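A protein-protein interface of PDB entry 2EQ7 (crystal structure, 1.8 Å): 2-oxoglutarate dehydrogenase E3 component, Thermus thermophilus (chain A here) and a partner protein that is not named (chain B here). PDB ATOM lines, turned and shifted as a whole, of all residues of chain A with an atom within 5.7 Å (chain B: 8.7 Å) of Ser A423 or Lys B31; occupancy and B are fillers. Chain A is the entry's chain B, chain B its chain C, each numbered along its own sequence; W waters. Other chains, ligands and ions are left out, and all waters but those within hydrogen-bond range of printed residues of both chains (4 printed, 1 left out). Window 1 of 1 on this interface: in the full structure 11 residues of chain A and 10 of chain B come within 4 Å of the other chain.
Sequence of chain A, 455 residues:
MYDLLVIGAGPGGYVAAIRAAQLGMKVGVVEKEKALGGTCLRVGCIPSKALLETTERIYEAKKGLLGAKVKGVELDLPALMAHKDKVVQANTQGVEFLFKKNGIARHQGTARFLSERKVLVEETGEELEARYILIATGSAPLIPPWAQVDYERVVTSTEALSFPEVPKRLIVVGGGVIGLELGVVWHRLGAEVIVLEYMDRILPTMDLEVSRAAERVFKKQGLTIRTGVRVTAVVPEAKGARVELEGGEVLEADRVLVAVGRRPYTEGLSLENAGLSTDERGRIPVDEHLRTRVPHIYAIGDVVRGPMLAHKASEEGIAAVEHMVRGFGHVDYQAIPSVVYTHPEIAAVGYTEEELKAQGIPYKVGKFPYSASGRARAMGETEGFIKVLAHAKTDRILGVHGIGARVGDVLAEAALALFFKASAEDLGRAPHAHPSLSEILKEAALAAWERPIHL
OE2 of Glu B32 sits close to OG1 of Thr A394 (3.5 Å). The side-chain carboxylate (OD1) of Asp A395 is in salt-bridge range of the side-chain amino group (NZ) of Lys B31 (2.9 Å). NH2 of Arg A396 lies within salt-bridge range of OE1 of Glu B32 (2.5 Å). OE1 of Glu A425 lies within salt-bridge range of NH2 of Arg B8 (2.6 Å). OE1 of Glu A425 is in salt-bridge range of NZ of Lys B31. The backbone NH (N) of Ala B5 sits at hydrogen-bond distance from the side-chain carboxylate (OD2) of Asp A426, 2.8 Å away.
The side-chain hydroxyl (OG1) of Thr A394 sits close to the backbone NH (N) of Arg A396 (3.2 Å). The backbone carbonyl oxygen of Asp A395 is in hydrogen-bond range of the backbone NH of Ala A424 (2.9 Å). The side-chain hydroxyl (OG) of Ser A423 sits close to the backbone NH (N) of Glu A425 (3.4 Å). OE1 of Glu A425 sits at hydrogen-bond distance from NE1 of Trp A449 (3.5 Å). N of Met B3 lies within hydrogen-bond range of O of Ile B29 (3.0 Å). The backbone NH (N) of Leu B30 lies within hydrogen-bond range of the side-chain carboxylate (OD2) of Asp B33 (2.7 Å).
Among the printed residues, merely in contact across the chains: Thr A394 with Lys B31, Arg A396 with Leu B30, Lys A421 with Leu B30, Ser A423 with Ala B5, Ser A423 with Lys B31, Glu A425 with Ala B5, Asp A426 with Met B3, Asp A426 with Pro B4 and Trp A449 with Lys B31.
Ser A423 touches just these residues of chain B: Ala B5 (3.8 Å) and Lys B31 (3.1 Å). Of the printed residues of chain A, Lys B31 touches Thr A394 (3.9 Å), Asp A395 (2.9 Å), Ser A423 (3.1 Å), Glu A425 (2.6 Å) and Trp A449 (3.6 Å). No residue of chain B comes within 4 Å of Ala A422. No residue of chain B comes within 4 Å of Ala A424. Of the printed residues of chain A, Arg B8 touches Glu A425 (2.6 Å). Printed residues of chain A within 4 Å of Met B3: Asp A426 (3.9 Å). Of the printed residues of chain B, Glu A425 touches Ala B5, Arg B8 and Lys B31. Of the printed residues of chain B, Arg A396 touches Leu B30 and Glu B32. Printed residues of chain A within 4 Å of Pro B4: Asp A426. Met B10 touches none of the printed residues of chain A. Ile B29 touches none of the printed residues of chain A. The nearest residue of chain B that does not touch Ser A423 is Met B3 (5.5 Å).
Of the 25 printed residues of chain B, 7 touch a printed residue of chain A. Hydrophobic or aromatic side chains of chain B within 4 Å of the printed part of chain A: Met B3, Pro B4, Ala B5 and Leu B30. Among the printed residues, 15 pairs touch across the chains. Among the printed residues, Asp or Glu carboxylates within 4 Å of a Lys or Arg side-chain nitrogen of the other chain: Asp A395 with Lys B31 (2.9 Å), Arg A396 with Glu B32 (2.5 Å), Glu A425 with Arg B8 (2.6 Å) and Glu A425 with Lys B31 (2.6 Å).
Water W2 bridges OG1 of Thr A394 and OE2 of Glu B32. Water W4 bridges NZ of Lys B31 and NE1 of Trp A449. Water W3 lies within hydrogen-bond range of N of Lys B31 and OD1 of Asp A426. Water W1 lies within hydrogen-bond range of NH2 of Arg A396 and O of Thr B23.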
ATOM      1  N   THR A 394      -2.552  -7.741  18.756  1.00  0.00           N
ATOM      2  CA  THR A 394      -2.796  -8.596  17.601  1.00  0.00           C
ATOM      3  C   THR A 394      -1.532  -9.166  16.958  1.00  0.00           C
ATOM      4  O   THR A 394      -1.612 -10.077  16.140  1.00  0.00           O
ATOM      5  CB  THR A 394      -3.553  -7.830  16.515  1.00  0.00           C
ATOM      6  OG1 THR A 394      -2.697  -6.815  15.971  1.00  0.00           O
ATOM      7  CG2 THR A 394      -4.800  -7.172  17.097  1.00  0.00           C
ATOM      8  N   ASP A 395      -0.377  -8.619  17.321  1.00  0.00           N
ATOM      9  CA  ASP A 395       0.907  -9.057  16.766  1.00  0.00           C
ATOM     10  C   ASP A 395       1.015  -8.707  15.281  1.00  0.00           C
ATOM     11  O   ASP A 395       1.968  -9.109  14.609  1.00  0.00           O
ATOM     12  CB  ASP A 395       1.096 -10.569  16.924  1.00  0.00           C
ATOM     13  CG  ASP A 395       2.536 -11.004  16.692  1.00  0.00           C
ATOM     14  OD1 ASP A 395       2.760 -12.074  16.085  1.00  0.00           O
ATOM     15  OD2 ASP A 395       3.446 -10.275  17.135  1.00  0.00           O
ATOM     16  N   ARG A 396       0.037  -7.972  14.759  1.00  0.00           N
ATOM     17  CA  ARG A 396       0.078  -7.596  13.349  1.00  0.00           C
ATOM     18  C   ARG A 396       1.287  -6.695  13.096  1.00  0.00           C
ATOM     19  O   ARG A 396       1.580  -5.810  13.897  1.00  0.00           O
ATOM     20  CB  ARG A 396      -1.205  -6.858  12.940  1.00  0.00           C
ATOM     21  CG  ARG A 396      -1.164  -6.360  11.499  1.00  0.00           C
ATOM     22  CD  ARG A 396      -2.421  -5.611  11.078  1.00  0.00           C
ATOM     23  NE  ARG A 396      -3.539  -6.501  10.775  1.00  0.00           N
ATOM     24  CZ  ARG A 396      -4.609  -6.135  10.076  1.00  0.00           C
ATOM     25  NH1 ARG A 396      -4.706  -4.899   9.606  1.00  0.00           N
ATOM     26  NH2 ARG A 396      -5.582  -7.005   9.837  1.00  0.00           N
ATOM     27  N   ILE A 397       2.000  -6.931  11.999  1.00  0.00           N
ATOM     28  CA  ILE A 397       3.158  -6.106  11.679  1.00  0.00           C
ATOM     29  C   ILE A 397       2.660  -4.710  11.316  1.00  0.00           C
ATOM     30  O   ILE A 397       1.784  -4.561  10.463  1.00  0.00           O
ATOM     31  CB  ILE A 397       3.958  -6.681  10.484  1.00  0.00           C
ATOM     32  CG1 ILE A 397       4.492  -8.076  10.835  1.00  0.00           C
ATOM     33  CG2 ILE A 397       5.124  -5.747  10.142  1.00  0.00           C
ATOM     34  CD1 ILE A 397       5.156  -8.789   9.666  1.00  0.00           C
ATOM     35  N   LYS A 421      -1.245  -8.380   5.461  1.00  0.00           N
ATOM     36  CA  LYS A 421      -1.664  -8.134   6.841  1.00  0.00           C
ATOM     37  C   LYS A 421      -1.101  -9.206   7.775  1.00  0.00           C
ATOM     38  O   LYS A 421      -1.766  -9.647   8.712  1.00  0.00           O
ATOM     39  CB  LYS A 421      -3.194  -8.120   6.935  1.00  0.00           C
ATOM     40  CG  LYS A 421      -3.862  -7.149   5.974  1.00  0.00           C
ATOM     41  CD  LYS A 421      -5.376  -7.155   6.135  1.00  0.00           C
ATOM     42  CE  LYS A 421      -6.048  -6.329   5.050  1.00  0.00           C
ATOM     43  NZ  LYS A 421      -5.532  -4.931   5.010  1.00  0.00           N
ATOM     44  N   ALA A 422       0.138  -9.609   7.518  1.00  0.00           N
ATOM     45  CA  ALA A 422       0.794 -10.639   8.313  1.00  0.00           C
ATOM     46  C   ALA A 422       1.159 -10.200   9.724  1.00  0.00           C
ATOM     47  O   ALA A 422       1.276  -9.011  10.017  1.00  0.00           O
ATOM     48  CB  ALA A 422       2.049 -11.128   7.590  1.00  0.00           C
ATOM     49  N   SER A 423       1.337 -11.182  10.599  1.00  0.00           N
ATOM     50  CA  SER A 423       1.725 -10.920  11.975  1.00  0.00           C
ATOM     51  C   SER A 423       3.226 -11.163  12.043  1.00  0.00           C
ATOM     52  O   SER A 423       3.804 -11.730  11.115  1.00  0.00           O
ATOM     53  CB  SER A 423       1.024 -11.891  12.921  1.00  0.00           C
ATOM     54  OG  SER A 423       1.455 -13.220  12.671  1.00  0.00           O
ATOM     55  N   ALA A 424       3.855 -10.736  13.132  1.00  0.00           N
ATOM     56  CA  ALA A 424       5.289 -10.941  13.295  1.00  0.00           C
ATOM     57  C   ALA A 424       5.560 -12.446  13.325  1.00  0.00           C
ATOM     58  O   ALA A 424       6.568 -12.921  12.798  1.00  0.00           O
ATOM     59  CB  ALA A 424       5.771 -10.290  14.580  1.00  0.00           C
ATOM     60  N   GLU A 425       4.648 -13.197  13.936  1.00  0.00           N
ATOM     61  CA  GLU A 425       4.795 -14.646  14.011  1.00  0.00           C
ATOM     62  C   GLU A 425       4.784 -15.265  12.614  1.00  0.00           C
ATOM     63  O   GLU A 425       5.579 -16.158  12.317  1.00  0.00           O
ATOM     64  CB  GLU A 425       3.668 -15.256  14.848  1.00  0.00           C
ATOM     65  CG  GLU A 425       3.696 -16.774  14.873  1.00  0.00           C
ATOM     66  CD  GLU A 425       2.559 -17.376  15.676  1.00  0.00           C
ATOM     67  OE1 GLU A 425       1.701 -16.612  16.166  1.00  0.00           O
ATOM     68  OE2 GLU A 425       2.522 -18.617  15.808  1.00  0.00           O
ATOM     69  N   ASP A 426       3.874 -14.795  11.768  1.00  0.00           N
ATOM     70  CA  ASP A 426       3.751 -15.289  10.399  1.00  0.00           C
ATOM     71  C   ASP A 426       5.065 -15.147   9.641  1.00  0.00           C
ATOM     72  O   ASP A 426       5.530 -16.092   9.001  1.00  0.00           O
ATOM     73  CB  ASP A 426       2.659 -14.514   9.658  1.00  0.00           C
ATOM     74  CG  ASP A 426       1.262 -14.912  10.094  1.00  0.00           C
ATOM     75  OD1 ASP A 426       0.382 -14.030  10.172  1.00  0.00           O
ATOM     76  OD2 ASP A 426       1.045 -16.113  10.343  1.00  0.00           O
ATOM     77  N   LEU A 427       5.654 -13.958   9.718  1.00  0.00           N
ATOM     78  CA  LEU A 427       6.913 -13.677   9.035  1.00  0.00           C
ATOM     79  C   LEU A 427       8.067 -14.443   9.670  1.00  0.00           C
ATOM     80  O   LEU A 427       8.894 -15.022   8.969  1.00  0.00           O
ATOM     81  CB  LEU A 427       7.202 -12.170   9.069  1.00  0.00           C
ATOM     82  CG  LEU A 427       8.498 -11.675   8.418  1.00  0.00           C
ATOM     83  CD1 LEU A 427       8.606 -12.204   6.990  1.00  0.00           C
ATOM     84  CD2 LEU A 427       8.517 -10.149   8.430  1.00  0.00           C
ATOM     85  N   GLY A 428       8.110 -14.457  10.999  1.00  0.00           N
ATOM     86  CA  GLY A 428       9.177 -15.154  11.695  1.00  0.00           C
ATOM     87  C   GLY A 428       9.175 -16.659  11.505  1.00  0.00           C
ATOM     88  O   GLY A 428      10.226 -17.297  11.554  1.00  0.00           O
ATOM     89  N   TRP A 449       7.608 -10.762  17.824  1.00  0.00           N
ATOM     90  CA  TRP A 449       6.555 -11.679  18.234  1.00  0.00           C
ATOM     91  C   TRP A 449       6.751 -12.163  19.666  1.00  0.00           C
ATOM     92  O   TRP A 449       5.821 -12.133  20.472  1.00  0.00           O
ATOM     93  CB  TRP A 449       6.516 -12.879  17.278  1.00  0.00           C
ATOM     94  CG  TRP A 449       5.631 -14.012  17.726  1.00  0.00           C
ATOM     95  CD1 TRP A 449       4.367 -13.915  18.233  1.00  0.00           C
ATOM     96  CD2 TRP A 449       5.937 -15.412  17.675  1.00  0.00           C
ATOM     97  NE1 TRP A 449       3.867 -15.169  18.501  1.00  0.00           N
ATOM     98  CE2 TRP A 449       4.809 -16.105  18.168  1.00  0.00           C
ATOM     99  CE3 TRP A 449       7.055 -16.149  17.259  1.00  0.00           C
ATOM    100  CZ2 TRP A 449       4.766 -17.503  18.258  1.00  0.00           C
ATOM    101  CZ3 TRP A 449       7.013 -17.541  17.349  1.00  0.00           C
ATOM    102  CH2 TRP A 449       5.873 -18.200  17.845  1.00  0.00           C
ATOM    103  N   ALA B   2      -6.307 -20.012   5.921  1.00  0.00           N
ATOM    104  CA  ALA B   2      -5.900 -18.940   6.820  1.00  0.00           C
ATOM    105  C   ALA B   2      -4.388 -18.754   6.840  1.00  0.00           C
ATOM    106  O   ALA B   2      -3.653 -19.436   6.120  1.00  0.00           O
ATOM    107  CB  ALA B   2      -6.405 -19.229   8.231  1.00  0.00           C
ATOM    108  N   MET B   3      -3.932 -17.819   7.666  1.00  0.00           N
ATOM    109  CA  MET B   3      -2.509 -17.544   7.799  1.00  0.00           C
ATOM    110  C   MET B   3      -1.893 -18.577   8.740  1.00  0.00           C
ATOM    111  O   MET B   3      -2.532 -19.012   9.700  1.00  0.00           O
ATOM    112  CB  MET B   3      -2.291 -16.133   8.354  1.00  0.00           C
ATOM    113  CG  MET B   3      -2.778 -15.019   7.447  1.00  0.00           C
ATOM    114  SD  MET B   3      -1.932 -15.030   5.858  1.00  0.00           S
ATOM    115  CE  MET B   3      -0.499 -13.994   6.220  1.00  0.00           C
ATOM    116  N   PRO B   4      -0.644 -18.985   8.471  1.00  0.00           N
ATOM    117  CA  PRO B   4       0.092 -19.972   9.269  1.00  0.00           C
ATOM    118  C   PRO B   4       0.031 -19.794  10.788  1.00  0.00           C
ATOM    119  O   PRO B   4      -0.083 -20.776  11.524  1.00  0.00           O
ATOM    120  CB  PRO B   4       1.509 -19.853   8.720  1.00  0.00           C
ATOM    121  CG  PRO B   4       1.258 -19.589   7.271  1.00  0.00           C
ATOM    122  CD  PRO B   4       0.167 -18.539   7.323  1.00  0.00           C
ATOM    123  N   ALA B   5       0.116 -18.554  11.263  1.00  0.00           N
ATOM    124  CA  ALA B   5       0.066 -18.295  12.699  1.00  0.00           C
ATOM    125  C   ALA B   5      -1.352 -18.477  13.232  1.00  0.00           C
ATOM    126  O   ALA B   5      -1.548 -18.830  14.396  1.00  0.00           O
ATOM    127  CB  ALA B   5       0.563 -16.884  13.003  1.00  0.00           C
ATOM    128  N   ALA B   6      -2.338 -18.231  12.376  1.00  0.00           N
ATOM    129  CA  ALA B   6      -3.736 -18.376  12.757  1.00  0.00           C
ATOM    130  C   ALA B   6      -4.041 -19.852  12.978  1.00  0.00           C
ATOM    131  O   ALA B   6      -4.725 -20.221  13.933  1.00  0.00           O
ATOM    132  CB  ALA B   6      -4.637 -17.814  11.666  1.00  0.00           C
ATOM    133  N   GLU B   7      -3.523 -20.690  12.085  1.00  0.00           N
ATOM    134  CA  GLU B   7      -3.723 -22.128  12.174  1.00  0.00           C
ATOM    135  C   GLU B   7      -3.057 -22.669  13.434  1.00  0.00           C
ATOM    136  O   GLU B   7      -3.558 -23.602  14.063  1.00  0.00           O
ATOM    137  CB  GLU B   7      -3.136 -22.817  10.940  1.00  0.00           C
ATOM    138  CG  GLU B   7      -3.811 -22.425   9.634  1.00  0.00           C
ATOM    139  CD  GLU B   7      -3.179 -23.089   8.427  1.00  0.00           C
ATOM    140  OE1 GLU B   7      -3.708 -22.918   7.308  1.00  0.00           O
ATOM    141  OE2 GLU B   7      -2.152 -23.782   8.596  1.00  0.00           O
ATOM    142  N   ARG B   8      -1.925 -22.073  13.796  1.00  0.00           N
ATOM    143  CA  ARG B   8      -1.184 -22.483  14.982  1.00  0.00           C
ATOM    144  C   ARG B   8      -1.987 -22.132  16.232  1.00  0.00           C
ATOM    145  O   ARG B   8      -2.031 -22.905  17.192  1.00  0.00           O
ATOM    146  CB  ARG B   8       0.182 -21.783  15.012  1.00  0.00           C
ATOM    147  CG  ARG B   8       1.093 -22.184  16.172  1.00  0.00           C
ATOM    148  CD  ARG B   8       0.700 -21.503  17.478  1.00  0.00           C
ATOM    149  NE  ARG B   8       0.826 -20.049  17.399  1.00  0.00           N
ATOM    150  CZ  ARG B   8       0.533 -19.216  18.395  1.00  0.00           C
ATOM    151  NH1 ARG B   8       0.094 -19.691  19.552  1.00  0.00           N
ATOM    152  NH2 ARG B   8       0.680 -17.908  18.235  1.00  0.00           N
ATOM    153  N   LEU B   9      -2.624 -20.966  16.211  1.00  0.00           N
ATOM    154  CA  LEU B   9      -3.426 -20.511  17.340  1.00  0.00           C
ATOM    155  C   LEU B   9      -4.708 -21.327  17.476  1.00  0.00           C
ATOM    156  O   LEU B   9      -5.161 -21.605  18.586  1.00  0.00           O
ATOM    157  CB  LEU B   9      -3.774 -19.028  17.175  1.00  0.00           C
ATOM    158  CG  LEU B   9      -4.561 -18.376  18.317  1.00  0.00           C
ATOM    159  CD1 LEU B   9      -3.763 -18.463  19.609  1.00  0.00           C
ATOM    160  CD2 LEU B   9      -4.856 -16.923  17.970  1.00  0.00           C
ATOM    161  N   MET B  10      -5.291 -21.708  16.343  1.00  0.00           N
ATOM    162  CA  MET B  10      -6.522 -22.491  16.345  1.00  0.00           C
ATOM    163  C   MET B  10      -6.286 -23.920  16.823  1.00  0.00           C
ATOM    164  O   MET B  10      -7.109 -24.483  17.543  1.00  0.00           O
ATOM    165  CB  MET B  10      -7.145 -22.519  14.946  1.00  0.00           C
ATOM    166  CG  MET B  10      -7.672 -21.176  14.466  1.00  0.00           C
ATOM    167  SD  MET B  10      -8.544 -21.296  12.889  1.00  0.00           S
ATOM    168  CE  MET B  10      -7.183 -21.111  11.733  1.00  0.00           C
ATOM    169  N   LYS B  13      -5.982 -23.766  20.781  1.00  0.00           N
ATOM    170  CA  LYS B  13      -7.250 -23.509  21.455  1.00  0.00           C
ATOM    171  C   LYS B  13      -8.350 -24.421  20.920  1.00  0.00           C
ATOM    172  O   LYS B  13      -9.516 -24.283  21.293  1.00  0.00           O
ATOM    173  CB  LYS B  13      -7.664 -22.046  21.271  1.00  0.00           C
ATOM    174  CG  LYS B  13      -6.667 -21.040  21.826  1.00  0.00           C
ATOM    175  CD  LYS B  13      -7.201 -19.617  21.729  1.00  0.00           C
ATOM    176  CE  LYS B  13      -7.487 -19.219  20.288  1.00  0.00           C
ATOM    177  NZ  LYS B  13      -8.059 -17.846  20.190  1.00  0.00           N
ATOM    178  N   VAL B  20     -14.137 -19.082  12.654  1.00  0.00           N
ATOM    179  CA  VAL B  20     -13.574 -17.738  12.593  1.00  0.00           C
ATOM    180  C   VAL B  20     -13.811 -17.075  11.240  1.00  0.00           C
ATOM    181  O   VAL B  20     -13.715 -17.719  10.195  1.00  0.00           O
ATOM    182  CB  VAL B  20     -12.054 -17.763  12.867  1.00  0.00           C
ATOM    183  CG1 VAL B  20     -11.510 -16.345  12.912  1.00  0.00           C
ATOM    184  CG2 VAL B  20     -11.773 -18.486  14.176  1.00  0.00           C
ATOM    185  N   GLN B  21     -14.120 -15.783  11.269  1.00  0.00           N
ATOM    186  CA  GLN B  21     -14.364 -15.021  10.051  1.00  0.00           C
ATOM    187  C   GLN B  21     -13.072 -14.328   9.622  1.00  0.00           C
ATOM    188  O   GLN B  21     -12.565 -13.452  10.321  1.00  0.00           O
ATOM    189  CB  GLN B  21     -15.462 -13.979  10.291  1.00  0.00           C
ATOM    190  CG  GLN B  21     -15.857 -13.191   9.051  1.00  0.00           C
ATOM    191  CD  GLN B  21     -16.984 -12.207   9.316  1.00  0.00           C
ATOM    192  OE1 GLN B  21     -17.432 -11.500   8.411  1.00  0.00           O
ATOM    193  NE2 GLN B  21     -17.448 -12.157  10.560  1.00  0.00           N
ATOM    194  N   GLY B  22     -12.545 -14.729   8.469  1.00  0.00           N
ATOM    195  CA  GLY B  22     -11.311 -14.148   7.976  1.00  0.00           C
ATOM    196  C   GLY B  22     -11.439 -12.718   7.487  1.00  0.00           C
ATOM    197  O   GLY B  22     -12.338 -12.394   6.710  1.00  0.00           O
ATOM    198  N   THR B  23     -10.533 -11.860   7.947  1.00  0.00           N
ATOM    199  CA  THR B  23     -10.530 -10.456   7.551  1.00  0.00           C
ATOM    200  C   THR B  23      -9.226 -10.132   6.829  1.00  0.00           C
ATOM    201  O   THR B  23      -8.946  -8.973   6.520  1.00  0.00           O
ATOM    202  CB  THR B  23     -10.670  -9.519   8.772  1.00  0.00           C
ATOM    203  OG1 THR B  23      -9.533  -9.672   9.633  1.00  0.00           O
ATOM    204  CG2 THR B  23     -11.939  -9.841   9.549  1.00  0.00           C
ATOM    205  N   GLY B  24      -8.432 -11.165   6.568  1.00  0.00           N
ATOM    206  CA  GLY B  24      -7.171 -10.971   5.878  1.00  0.00           C
ATOM    207  C   GLY B  24      -7.391 -10.792   4.390  1.00  0.00           C
ATOM    208  O   GLY B  24      -8.533 -10.800   3.924  1.00  0.00           O
ATOM    209  N   ARG B  28      -8.765 -15.235   4.015  1.00  0.00           N
ATOM    210  CA  ARG B  28      -7.715 -15.695   4.920  1.00  0.00           C
ATOM    211  C   ARG B  28      -7.985 -15.242   6.349  1.00  0.00           C
ATOM    212  O   ARG B  28      -8.273 -14.071   6.598  1.00  0.00           O
ATOM    213  CB  ARG B  28      -6.355 -15.159   4.471  1.00  0.00           C
ATOM    214  CG  ARG B  28      -5.966 -15.553   3.060  1.00  0.00           C
ATOM    215  CD  ARG B  28      -4.668 -14.884   2.644  1.00  0.00           C
ATOM    216  NE  ARG B  28      -4.318 -15.192   1.260  1.00  0.00           N
ATOM    217  CZ  ARG B  28      -3.247 -14.715   0.636  1.00  0.00           C
ATOM    218  NH1 ARG B  28      -3.009 -15.051  -0.625  1.00  0.00           N
ATOM    219  NH2 ARG B  28      -2.412 -13.902   1.271  1.00  0.00           N
ATOM    220  N   ILE B  29      -7.885 -16.178   7.286  1.00  0.00           N
ATOM    221  CA  ILE B  29      -8.110 -15.878   8.693  1.00  0.00           C
ATOM    222  C   ILE B  29      -6.802 -15.475   9.365  1.00  0.00           C
ATOM    223  O   ILE B  29      -5.851 -16.255   9.407  1.00  0.00           O
ATOM    224  CB  ILE B  29      -8.695 -17.099   9.442  1.00  0.00           C
ATOM    225  CG1 ILE B  29     -10.065 -17.459   8.863  1.00  0.00           C
ATOM    226  CG2 ILE B  29      -8.809 -16.795  10.927  1.00  0.00           C
ATOM    227  CD1 ILE B  29     -10.703 -18.678   9.502  1.00  0.00           C
ATOM    228  N   LEU B  30      -6.760 -14.252   9.881  1.00  0.00           N
ATOM    229  CA  LEU B  30      -5.572 -13.749  10.561  1.00  0.00           C
ATOM    230  C   LEU B  30      -5.595 -14.245  12.003  1.00  0.00           C
ATOM    231  O   LEU B  30      -6.663 -14.516  12.552  1.00  0.00           O
ATOM    232  CB  LEU B  30      -5.556 -12.218  10.539  1.00  0.00           C
ATOM    233  CG  LEU B  30      -5.613 -11.548   9.163  1.00  0.00           C
ATOM    234  CD1 LEU B  30      -5.676 -10.039   9.335  1.00  0.00           C
ATOM    235  CD2 LEU B  30      -4.395 -11.941   8.340  1.00  0.00           C
ATOM    236  N   LYS B  31      -4.421 -14.365  12.613  1.00  0.00           N
ATOM    237  CA  LYS B  31      -4.335 -14.835  13.991  1.00  0.00           C
ATOM    238  C   LYS B  31      -5.115 -13.920  14.929  1.00  0.00           C
ATOM    239  O   LYS B  31      -5.522 -14.333  16.016  1.00  0.00           O
ATOM    240  CB  LYS B  31      -2.872 -14.911  14.439  1.00  0.00           C
ATOM    241  CG  LYS B  31      -2.148 -13.581  14.417  1.00  0.00           C
ATOM    242  CD  LYS B  31      -0.686 -13.733  14.806  1.00  0.00           C
ATOM    243  CE  LYS B  31      -0.515 -14.183  16.244  1.00  0.00           C
ATOM    244  NZ  LYS B  31       0.924 -14.195  16.627  1.00  0.00           N
ATOM    245  N   GLU B  32      -5.324 -12.677  14.505  1.00  0.00           N
ATOM    246  CA  GLU B  32      -6.066 -11.719  15.314  1.00  0.00           C
ATOM    247  C   GLU B  32      -7.561 -12.007  15.216  1.00  0.00           C
ATOM    248  O   GLU B  32      -8.339 -11.604  16.081  1.00  0.00           O
ATOM    249  CB  GLU B  32      -5.775 -10.289  14.852  1.00  0.00           C
ATOM    250  CG  GLU B  32      -6.270  -9.966  13.455  1.00  0.00           C
ATOM    251  CD  GLU B  32      -5.910  -8.556  13.022  1.00  0.00           C
ATOM    252  OE1 GLU B  32      -6.351  -8.140  11.932  1.00  0.00           O
ATOM    253  OE2 GLU B  32      -5.184  -7.866  13.769  1.00  0.00           O
ATOM    254  N   ASP B  33      -7.955 -12.706  14.155  1.00  0.00           N
ATOM    255  CA  ASP B  33      -9.355 -13.063  13.953  1.00  0.00           C
ATOM    256  C   ASP B  33      -9.723 -14.213  14.884  1.00  0.00           C
ATOM    257  O   ASP B  33     -10.847 -14.290  15.379  1.00  0.00           O
ATOM    258  CB  ASP B  33      -9.601 -13.484  12.500  1.00  0.00           C
ATOM    259  CG  ASP B  33      -9.421 -12.340  11.522  1.00  0.00           C
ATOM    260  OD1 ASP B  33     -10.100 -11.303  11.685  1.00  0.00           O
ATOM    261  OD2 ASP B  33      -8.606 -12.479  10.586  1.00  0.00           O
ATOM    262  N   VAL B  34      -8.761 -15.103  15.114  1.00  0.00           N
ATOM    263  CA  VAL B  34      -8.966 -16.253  15.985  1.00  0.00           C
ATOM    264  C   VAL B  34      -9.103 -15.795  17.434  1.00  0.00           C
ATOM    265  O   VAL B  34     -10.062 -16.151  18.118  1.00  0.00           O
ATOM    266  CB  VAL B  34      -7.785 -17.243  15.887  1.00  0.00           C
ATOM    267  CG1 VAL B  34      -8.045 -18.453  16.773  1.00  0.00           C
ATOM    268  CG2 VAL B  34      -7.588 -17.674  14.442  1.00  0.00           C
ATOM    269  N   MET B  35      -8.138 -15.005  17.894  1.00  0.00           N
ATOM    270  CA  MET B  35      -8.161 -14.498  19.260  1.00  0.00           C
ATOM    271  C   MET B  35      -9.356 -13.571  19.452  1.00  0.00           C
ATOM    272  O   MET B  35      -9.677 -13.176  20.572  1.00  0.00           O
ATOM    273  CB  MET B  35      -6.861 -13.752  19.575  1.00  0.00           C
ATOM    274  CG  MET B  35      -6.564 -12.581  18.652  1.00  0.00           C
ATOM    275  SD  MET B  35      -5.016 -11.747  19.073  1.00  0.00           S
ATOM    276  CE  MET B  35      -5.617 -10.436  20.138  1.00  0.00           C
ATOM    277  N   ARG B  36     -10.009 -13.230  18.345  1.00  0.00           N
ATOM    278  CA  ARG B  36     -11.178 -12.360  18.376  1.00  0.00           C
ATOM    279  C   ARG B  36     -12.401 -13.172  18.788  1.00  0.00           C
ATOM    280  O   ARG B  36     -13.342 -12.642  19.381  1.00  0.00           O
ATOM    281  CB  ARG B  36     -11.411 -11.745  16.994  1.00  0.00           C
ATOM    282  CG  ARG B  36     -12.604 -10.810  16.916  1.00  0.00           C
ATOM    283  CD  ARG B  36     -12.838 -10.361  15.485  1.00  0.00           C
ATOM    284  NE  ARG B  36     -13.123 -11.494  14.609  1.00  0.00           N
ATOM    285  CZ  ARG B  36     -13.244 -11.409  13.288  1.00  0.00           C
ATOM    286  NH1 ARG B  36     -13.101 -10.239  12.681  1.00  0.00           N
ATOM    287  NH2 ARG B  36     -13.510 -12.493  12.575  1.00  0.00           N
ATOM    288  N   HIS B  37     -12.377 -14.461  18.468  1.00  0.00           N
ATOM    289  CA  HIS B  37     -13.475 -15.359  18.805  1.00  0.00           C
ATOM    290  C   HIS B  37     -13.165 -16.114  20.093  1.00  0.00           C
ATOM    291  O   HIS B  37     -13.940 -15.963  21.060  1.00  0.00           O
ATOM    292  CB  HIS B  37     -13.711 -16.342  17.664  1.00  0.00           C
HETATM  293  O   HOH W   1      -7.948  -6.305   7.957  1.00  0.00           O
HETATM  294  O   HOH W   2      -4.076  -5.095  14.430  1.00  0.00           O
HETATM  295  O   HOH W   3      -2.171 -13.417  11.271  1.00  0.00           O
HETATM  296  O   HOH W   4       0.887 -13.998  19.357  1.00  0.00           O
